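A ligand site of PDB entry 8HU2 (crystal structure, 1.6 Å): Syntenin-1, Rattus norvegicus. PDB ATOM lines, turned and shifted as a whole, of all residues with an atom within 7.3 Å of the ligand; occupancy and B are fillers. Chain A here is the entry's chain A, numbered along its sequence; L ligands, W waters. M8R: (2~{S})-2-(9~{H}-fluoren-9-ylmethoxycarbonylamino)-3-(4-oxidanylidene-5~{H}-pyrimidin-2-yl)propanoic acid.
The backbone NH of Gly 101 is in hydrogen-bond range of an oxygen (O11) of the ligand, at 2.6 Å. The backbone NH (N) of Val 100 sits at hydrogen-bond distance from an oxygen (O12) of the ligand (2.8 Å). O11 of the ligand is in hydrogen-bond range of N of Phe 102, 3.2 Å away. N13 of the ligand lies within hydrogen-bond range of O of Phe 102 (3.3 Å). The backbone NH (N) of Phe 104 is in hydrogen-bond range of an oxygen (O03) of the ligand (3.2 Å).
O of Gly 101 is in hydrogen-bond range of N of Val 113, 2.9 Å away. The side-chain hydroxyl (OG) of Ser 116 lies within hydrogen-bond range of the backbone carbonyl oxygen (O) of Gly 101, at 3.4 Å. The backbone carbonyl oxygen of Val 100 is in hydrogen-bond range of the backbone NH of Ala 118 (2.8 Å). N of His 99 sits at hydrogen-bond distance from OD1 of Asp 95 (2.9 Å). The backbone carbonyl oxygen (O) of Ser 97 sits at hydrogen-bond distance from a ring nitrogen (NE2) of His 99 (3.5 Å). The backbone carbonyl oxygen (O) of Ile 103 sits at hydrogen-bond distance from the backbone NH (N) of Thr 110 (2.8 Å). O of Val 113 sits at hydrogen-bond distance from OG of Ser 116 (2.7 Å).
CA of His 99 touches O12 of the ligand, at 3.3 Å. Ile 103 touches the ligand. CG1 of Val 113 touches C21 of the ligand (3.9 Å). Ala 146 touches the ligand. Hydrophobic or aromatic side chains within 4 Å of the ligand: His 99, Val 100, Ile 103, Phe 104, Val 113 and Ala 146. Within 4 Å of the ligand: His 99, Val 100, Gly 101, Phe 102, Ile 103, Phe 104, Val 113 and Ala 146.
Water W1 bridges N06 of the ligand (3.0 Å) and O of Ala 146 (3.1 Å).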
ATOM      1  N   LYS A  94      -7.219  15.543  -9.961  1.00  0.00           N
ATOM      2  CA  LYS A  94      -6.223  14.575  -9.516  1.00  0.00           C
ATOM      3  C   LYS A  94      -6.311  13.307 -10.354  1.00  0.00           C
ATOM      4  O   LYS A  94      -7.394  12.815 -10.659  1.00  0.00           O
ATOM      5  CB  LYS A  94      -6.415  14.225  -8.039  1.00  0.00           C
ATOM      6  CG  LYS A  94      -6.086  15.376  -7.101  1.00  0.00           C
ATOM      7  CD  LYS A  94      -6.282  14.967  -5.633  1.00  0.00           C
ATOM      8  CE  LYS A  94      -5.828  16.064  -4.718  1.00  0.00           C
ATOM      9  NZ  LYS A  94      -5.842  15.612  -3.275  1.00  0.00           N
ATOM     10  N   ASP A  95      -5.144  12.779 -10.732  1.00  0.00           N
ATOM     11  CA  ASP A  95      -5.125  11.506 -11.439  1.00  0.00           C
ATOM     12  C   ASP A  95      -5.235  10.363 -10.430  1.00  0.00           C
ATOM     13  O   ASP A  95      -5.425  10.569  -9.225  1.00  0.00           O
ATOM     14  CB  ASP A  95      -3.894  11.415 -12.333  1.00  0.00           C
ATOM     15  CG  ASP A  95      -2.577  11.241 -11.577  1.00  0.00           C
ATOM     16  OD1 ASP A  95      -2.535  11.148 -10.322  1.00  0.00           O
ATOM     17  OD2 ASP A  95      -1.541  11.181 -12.271  1.00  0.00           O
ATOM     18  N   SER A  97      -3.086   8.436  -9.128  1.00  0.00           N
ATOM     19  CA  SER A  97      -2.096   8.479  -8.061  1.00  0.00           C
ATOM     20  C   SER A  97      -2.275   9.658  -7.122  1.00  0.00           C
ATOM     21  O   SER A  97      -1.462   9.842  -6.211  1.00  0.00           O
ATOM     22  CB  SER A  97      -0.672   8.521  -8.636  1.00  0.00           C
ATOM     23  OG  SER A  97      -0.406   7.355  -9.396  1.00  0.00           O
ATOM     24  N   GLY A  98      -3.329  10.464  -7.324  1.00  0.00           N
ATOM     25  CA  GLY A  98      -3.582  11.591  -6.456  1.00  0.00           C
ATOM     26  C   GLY A  98      -2.861  12.870  -6.806  1.00  0.00           C
ATOM     27  O   GLY A  98      -2.807  13.792  -5.986  1.00  0.00           O
ATOM     28  N   HIS A  99      -2.299  12.973  -8.020  1.00  0.00           N
ATOM     29  CA  HIS A  99      -1.459  14.095  -8.405  1.00  0.00           C
ATOM     30  C   HIS A  99      -2.161  15.023  -9.385  1.00  0.00           C
ATOM     31  O   HIS A  99      -2.835  14.554 -10.318  1.00  0.00           O
ATOM     32  CB  HIS A  99      -0.156  13.618  -9.058  1.00  0.00           C
ATOM     33  CG  HIS A  99       0.598  12.615  -8.248  1.00  0.00           C
ATOM     34  ND1 HIS A  99       1.156  11.479  -8.793  1.00  0.00           N
ATOM     35  CD2 HIS A  99       0.883  12.578  -6.924  1.00  0.00           C
ATOM     36  CE1 HIS A  99       1.765  10.786  -7.854  1.00  0.00           C
ATOM     37  NE2 HIS A  99       1.613  11.426  -6.707  1.00  0.00           N
ATOM     38  N   VAL A 100      -1.947  16.320  -9.224  1.00  0.00           N
ATOM     39  CA  VAL A 100      -2.421  17.272 -10.242  1.00  0.00           C
ATOM     40  C   VAL A 100      -1.306  17.648 -11.208  1.00  0.00           C
ATOM     41  O   VAL A 100      -1.583  17.951 -12.366  1.00  0.00           O
ATOM     42  CB  VAL A 100      -3.029  18.540  -9.618  1.00  0.00           C
ATOM     43  CG1 VAL A 100      -4.460  18.244  -9.140  1.00  0.00           C
ATOM     44  CG2 VAL A 100      -2.183  19.048  -8.491  1.00  0.00           C
ATOM     45  N   GLY A 101      -0.051  17.639 -10.755  1.00  0.00           N
ATOM     46  CA  GLY A 101       1.080  17.777 -11.679  1.00  0.00           C
ATOM     47  C   GLY A 101       1.901  19.046 -11.652  1.00  0.00           C
ATOM     48  O   GLY A 101       2.273  19.562 -12.715  1.00  0.00           O
ATOM     49  N   PHE A 102       2.225  19.593 -10.474  1.00  0.00           N
ATOM     50  CA  PHE A 102       3.118  20.745 -10.479  1.00  0.00           C
ATOM     51  C   PHE A 102       4.011  20.700  -9.253  1.00  0.00           C
ATOM     52  O   PHE A 102       3.697  20.081  -8.234  1.00  0.00           O
ATOM     53  CB  PHE A 102       2.363  22.077 -10.545  1.00  0.00           C
ATOM     54  CG  PHE A 102       1.469  22.363  -9.345  1.00  0.00           C
ATOM     55  CD1 PHE A 102       0.149  21.928  -9.331  1.00  0.00           C
ATOM     56  CD2 PHE A 102       1.945  23.098  -8.274  1.00  0.00           C
ATOM     57  CE1 PHE A 102      -0.668  22.211  -8.244  1.00  0.00           C
ATOM     58  CE2 PHE A 102       1.135  23.375  -7.185  1.00  0.00           C
ATOM     59  CZ  PHE A 102      -0.178  22.931  -7.170  1.00  0.00           C
ATOM     60  N   ILE A 103       5.147  21.385  -9.381  1.00  0.00           N
ATOM     61  CA  ILE A 103       6.117  21.574  -8.310  1.00  0.00           C
ATOM     62  C   ILE A 103       6.058  23.047  -7.902  1.00  0.00           C
ATOM     63  O   ILE A 103       5.884  23.919  -8.747  1.00  0.00           O
ATOM     64  CB  ILE A 103       7.532  21.202  -8.790  1.00  0.00           C
ATOM     65  CG1 ILE A 103       7.549  19.756  -9.303  1.00  0.00           C
ATOM     66  CG2 ILE A 103       8.576  21.448  -7.699  1.00  0.00           C
ATOM     67  CD1 ILE A 103       7.261  18.718  -8.240  1.00  0.00           C
ATOM     68  N   PHE A 104       6.197  23.308  -6.610  1.00  0.00           N
ATOM     69  CA  PHE A 104       6.204  24.684  -6.155  1.00  0.00           C
ATOM     70  C   PHE A 104       7.251  24.850  -5.071  1.00  0.00           C
ATOM     71  O   PHE A 104       7.666  23.877  -4.435  1.00  0.00           O
ATOM     72  CB  PHE A 104       4.829  25.140  -5.640  1.00  0.00           C
ATOM     73  CG  PHE A 104       4.369  24.440  -4.391  1.00  0.00           C
ATOM     74  CD1 PHE A 104       3.699  23.220  -4.458  1.00  0.00           C
ATOM     75  CD2 PHE A 104       4.581  25.007  -3.134  1.00  0.00           C
ATOM     76  CE1 PHE A 104       3.270  22.583  -3.333  1.00  0.00           C
ATOM     77  CE2 PHE A 104       4.146  24.381  -1.990  1.00  0.00           C
ATOM     78  CZ  PHE A 104       3.490  23.155  -2.087  1.00  0.00           C
ATOM     79  N   LYS A 105       7.695  26.088  -4.892  1.00  0.00           N
ATOM     80  CA  LYS A 105       8.666  26.423  -3.857  1.00  0.00           C
ATOM     81  C   LYS A 105       8.363  27.815  -3.330  1.00  0.00           C
ATOM     82  O   LYS A 105       8.157  28.750  -4.115  1.00  0.00           O
ATOM     83  CB  LYS A 105      10.098  26.352  -4.412  1.00  0.00           C
ATOM     84  CG  LYS A 105      11.163  26.853  -3.459  1.00  0.00           C
ATOM     85  CD  LYS A 105      12.179  25.759  -3.154  1.00  0.00           C
ATOM     86  CE  LYS A 105      13.105  26.164  -2.019  1.00  0.00           C
ATOM     87  NZ  LYS A 105      12.359  26.702  -0.856  1.00  0.00           N
ATOM     88  N   THR A 110       6.725  26.357  -9.815  1.00  0.00           N
ATOM     89  CA  THR A 110       8.028  26.396 -10.479  1.00  0.00           C
ATOM     90  C   THR A 110       8.149  25.462 -11.674  1.00  0.00           C
ATOM     91  O   THR A 110       8.962  25.725 -12.565  1.00  0.00           O
ATOM     92  CB  THR A 110       9.153  26.075  -9.481  1.00  0.00           C
ATOM     93  OG1 THR A 110       8.889  24.841  -8.819  1.00  0.00           O
ATOM     94  CG2 THR A 110       9.283  27.195  -8.454  1.00  0.00           C
ATOM     95  N   VAL A 113       4.415  19.331 -14.581  1.00  0.00           N
ATOM     96  CA  VAL A 113       4.769  17.942 -14.875  1.00  0.00           C
ATOM     97  C   VAL A 113       4.184  17.565 -16.233  1.00  0.00           C
ATOM     98  O   VAL A 113       3.008  17.823 -16.518  1.00  0.00           O
ATOM     99  CB  VAL A 113       4.260  17.011 -13.767  1.00  0.00           C
ATOM    100  CG1 VAL A 113       4.510  15.546 -14.117  1.00  0.00           C
ATOM    101  CG2 VAL A 113       4.928  17.366 -12.427  1.00  0.00           C
ATOM    102  N   LYS A 114       5.002  16.915 -17.072  1.00  0.00           N
ATOM    103  CA  LYS A 114       4.559  16.534 -18.410  1.00  0.00           C
ATOM    104  C   LYS A 114       3.346  15.604 -18.349  1.00  0.00           C
ATOM    105  O   LYS A 114       3.310  14.653 -17.569  1.00  0.00           O
ATOM    106  CB  LYS A 114       5.708  15.847 -19.155  1.00  0.00           C
ATOM    107  CG  LYS A 114       5.435  15.597 -20.631  1.00  0.00           C
ATOM    108  CD  LYS A 114       6.635  14.930 -21.289  1.00  0.00           C
ATOM    109  CE  LYS A 114       6.475  14.940 -22.803  1.00  0.00           C
ATOM    110  NZ  LYS A 114       5.290  14.151 -23.194  1.00  0.00           N
ATOM    111  N   SER A 116       0.403  15.861 -17.260  1.00  0.00           N
ATOM    112  CA  SER A 116      -0.392  15.886 -16.045  1.00  0.00           C
ATOM    113  C   SER A 116      -1.648  16.736 -16.262  1.00  0.00           C
ATOM    114  O   SER A 116      -1.835  17.375 -17.289  1.00  0.00           O
ATOM    115  CB  SER A 116       0.424  16.478 -14.902  1.00  0.00           C
ATOM    116  OG  SER A 116       0.683  17.846 -15.221  1.00  0.00           O
ATOM    117  N   ALA A 118      -2.213  19.490 -14.645  1.00  0.00           N
ATOM    118  CA  ALA A 118      -1.712  20.860 -14.714  1.00  0.00           C
ATOM    119  C   ALA A 118      -1.271  21.215 -16.125  1.00  0.00           C
ATOM    120  O   ALA A 118      -1.515  22.331 -16.596  1.00  0.00           O
ATOM    121  CB  ALA A 118      -0.545  21.035 -13.745  1.00  0.00           C
ATOM    122  N   ASP A 142       5.471  25.776   2.813  1.00  0.00           N
ATOM    123  CA  ASP A 142       5.260  24.854   1.701  1.00  0.00           C
ATOM    124  C   ASP A 142       4.650  23.531   2.159  1.00  0.00           C
ATOM    125  O   ASP A 142       3.781  22.969   1.489  1.00  0.00           O
ATOM    126  CB  ASP A 142       6.576  24.606   0.966  1.00  0.00           C
ATOM    127  CG  ASP A 142       6.962  25.747   0.066  1.00  0.00           C
ATOM    128  OD1 ASP A 142       6.111  26.627  -0.223  1.00  0.00           O
ATOM    129  OD2 ASP A 142       8.131  25.785  -0.363  1.00  0.00           O
ATOM    130  N   ALA A 143       5.099  23.002   3.315  1.00  0.00           N
ATOM    131  CA  ALA A 143       4.521  21.756   3.810  1.00  0.00           C
ATOM    132  C   ALA A 143       3.044  21.926   4.144  1.00  0.00           C
ATOM    133  O   ALA A 143       2.269  20.976   3.989  1.00  0.00           O
ATOM    134  CB  ALA A 143       5.291  21.273   5.044  1.00  0.00           C
ATOM    135  N   ILE A 145       0.949  24.074   2.567  1.00  0.00           N
ATOM    136  CA  ILE A 145       0.295  24.091   1.262  1.00  0.00           C
ATOM    137  C   ILE A 145       0.158  22.676   0.715  1.00  0.00           C
ATOM    138  O   ILE A 145      -0.894  22.263   0.213  1.00  0.00           O
ATOM    139  CB  ILE A 145       1.064  24.996   0.287  1.00  0.00           C
ATOM    140  CG1 ILE A 145       1.083  26.447   0.799  1.00  0.00           C
ATOM    141  CG2 ILE A 145       0.442  24.959  -1.110  1.00  0.00           C
ATOM    142  CD1 ILE A 145       2.128  27.321   0.101  1.00  0.00           C
ATOM    143  N   ALA A 146       1.241  21.897   0.830  1.00  0.00           N
ATOM    144  CA  ALA A 146       1.220  20.538   0.312  1.00  0.00           C
ATOM    145  C   ALA A 146       0.177  19.695   1.025  1.00  0.00           C
ATOM    146  O   ALA A 146      -0.495  18.857   0.402  1.00  0.00           O
ATOM    147  CB  ALA A 146       2.616  19.910   0.447  1.00  0.00           C
ATOM    148  N   ASP A 147       0.009  19.910   2.330  1.00  0.00           N
ATOM    149  CA  ASP A 147      -0.986  19.172   3.085  1.00  0.00           C
ATOM    150  C   ASP A 147      -2.392  19.502   2.607  1.00  0.00           C
ATOM    151  O   ASP A 147      -3.215  18.602   2.433  1.00  0.00           O
ATOM    152  CB  ASP A 147      -0.829  19.483   4.581  1.00  0.00           C
ATOM    153  CG  ASP A 147      -2.008  19.002   5.425  1.00  0.00           C
ATOM    154  OD1 ASP A 147      -2.267  17.777   5.454  1.00  0.00           O
ATOM    155  OD2 ASP A 147      -2.660  19.849   6.053  1.00  0.00           O
ATOM    156  N   LEU A 149      -3.293  20.670  -0.334  1.00  0.00           N
ATOM    157  CA  LEU A 149      -3.431  20.040  -1.641  1.00  0.00           C
ATOM    158  C   LEU A 149      -3.719  18.546  -1.512  1.00  0.00           C
ATOM    159  O   LEU A 149      -4.600  18.013  -2.188  1.00  0.00           O
ATOM    160  CB  LEU A 149      -2.154  20.244  -2.477  1.00  0.00           C
ATOM    161  CG  LEU A 149      -1.928  21.552  -3.212  1.00  0.00           C
ATOM    162  CD1 LEU A 149      -0.495  21.627  -3.722  1.00  0.00           C
ATOM    163  CD2 LEU A 149      -2.929  21.701  -4.374  1.00  0.00           C
ATOM    164  N   SER A 150      -2.975  17.873  -0.629  1.00  0.00           N
ATOM    165  CA  SER A 150      -3.062  16.418  -0.540  1.00  0.00           C
ATOM    166  C   SER A 150      -4.425  15.957  -0.044  1.00  0.00           C
ATOM    167  O   SER A 150      -4.923  14.913  -0.480  1.00  0.00           O
ATOM    168  CB  SER A 150      -1.942  15.886   0.363  1.00  0.00           C
ATOM    169  OG  SER A 150      -2.075  14.494   0.584  1.00  0.00           O
ATOM    170  N   VAL A 156      -9.414  20.171  -8.140  1.00  0.00           N
ATOM    171  CA  VAL A 156      -8.476  21.082  -7.472  1.00  0.00           C
ATOM    172  C   VAL A 156      -8.449  22.375  -8.273  1.00  0.00           C
ATOM    173  O   VAL A 156      -7.840  22.436  -9.349  1.00  0.00           O
ATOM    174  CB  VAL A 156      -7.071  20.490  -7.334  1.00  0.00           C
ATOM    175  CG1 VAL A 156      -6.142  21.479  -6.629  1.00  0.00           C
ATOM    176  CG2 VAL A 156      -7.121  19.168  -6.578  1.00  0.00           C
HETATM  177  C10 M8R L   1       0.825  17.166  -7.278  1.00  0.00           C
HETATM  178  C17 M8R L   1       5.483  14.283  -6.680  1.00  0.00           C
HETATM  179  C20 M8R L   1       3.551  14.198  -9.383  1.00  0.00           C
HETATM  180  C21 M8R L   1       3.321  13.966 -10.741  1.00  0.00           C
HETATM  181  C22 M8R L   1       3.726  12.750 -11.341  1.00  0.00           C
HETATM  182  C24 M8R L   1       5.233  11.834  -6.929  1.00  0.00           C
HETATM  183  C26 M8R L   1       4.590  12.001  -9.196  1.00  0.00           C
HETATM  184  C28 M8R L   1       6.336   9.964  -5.867  1.00  0.00           C
HETATM  185  C02 M8R L   1       5.170  20.000  -4.591  1.00  0.00           C
HETATM  186  C04 M8R L   1       5.188  19.628  -3.255  1.00  0.00           C
HETATM  187  C05 M8R L   1       4.057  18.996  -2.751  1.00  0.00           C
HETATM  188  C07 M8R L   1       3.053  19.141  -4.816  1.00  0.00           C
HETATM  189  C08 M8R L   1       1.838  18.854  -5.704  1.00  0.00           C
HETATM  190  C09 M8R L   1       1.862  17.406  -6.187  1.00  0.00           C
HETATM  191  C14 M8R L   1       3.908  15.993  -6.295  1.00  0.00           C
HETATM  192  C18 M8R L   1       4.569  13.154  -7.157  1.00  0.00           C
HETATM  193  C19 M8R L   1       4.193  13.223  -8.607  1.00  0.00           C
HETATM  194  C23 M8R L   1       4.368  11.775 -10.565  1.00  0.00           C
HETATM  195  C25 M8R L   1       5.234  11.154  -8.148  1.00  0.00           C
HETATM  196  C27 M8R L   1       5.777  11.241  -5.783  1.00  0.00           C
HETATM  197  C29 M8R L   1       6.351   9.282  -7.096  1.00  0.00           C
HETATM  198  C30 M8R L   1       5.800   9.873  -8.221  1.00  0.00           C
HETATM  199  N01 M8R L   1       4.105  19.738  -5.333  1.00  0.00           N
HETATM  200  N06 M8R L   1       3.022  18.768  -3.540  1.00  0.00           N
HETATM  201  N13 M8R L   1       3.163  17.147  -6.746  1.00  0.00           N
HETATM  202  O03 M8R L   1       6.112  20.544  -5.077  1.00  0.00           O
HETATM  203  O11 M8R L   1       1.143  17.349  -8.483  1.00  0.00           O
HETATM  204  O12 M8R L   1      -0.328  16.782  -6.961  1.00  0.00           O
HETATM  205  O15 M8R L   1       3.627  15.474  -5.264  1.00  0.00           O
HETATM  206  O16 M8R L   1       4.955  15.521  -7.078  1.00  0.00           O
HETATM  207  O   HOH W   1       0.543  17.668  -2.254  1.00  0.00           O
HETATM  208  O   HOH W   2       8.768  20.370  -4.196  1.00  0.00           O
HETATM  209  O   HOH W   3       0.709  13.724 -12.969  1.00  0.00           O
HETATM  210  O   HOH W   4      -0.749  15.919  -3.732  1.00  0.00           O
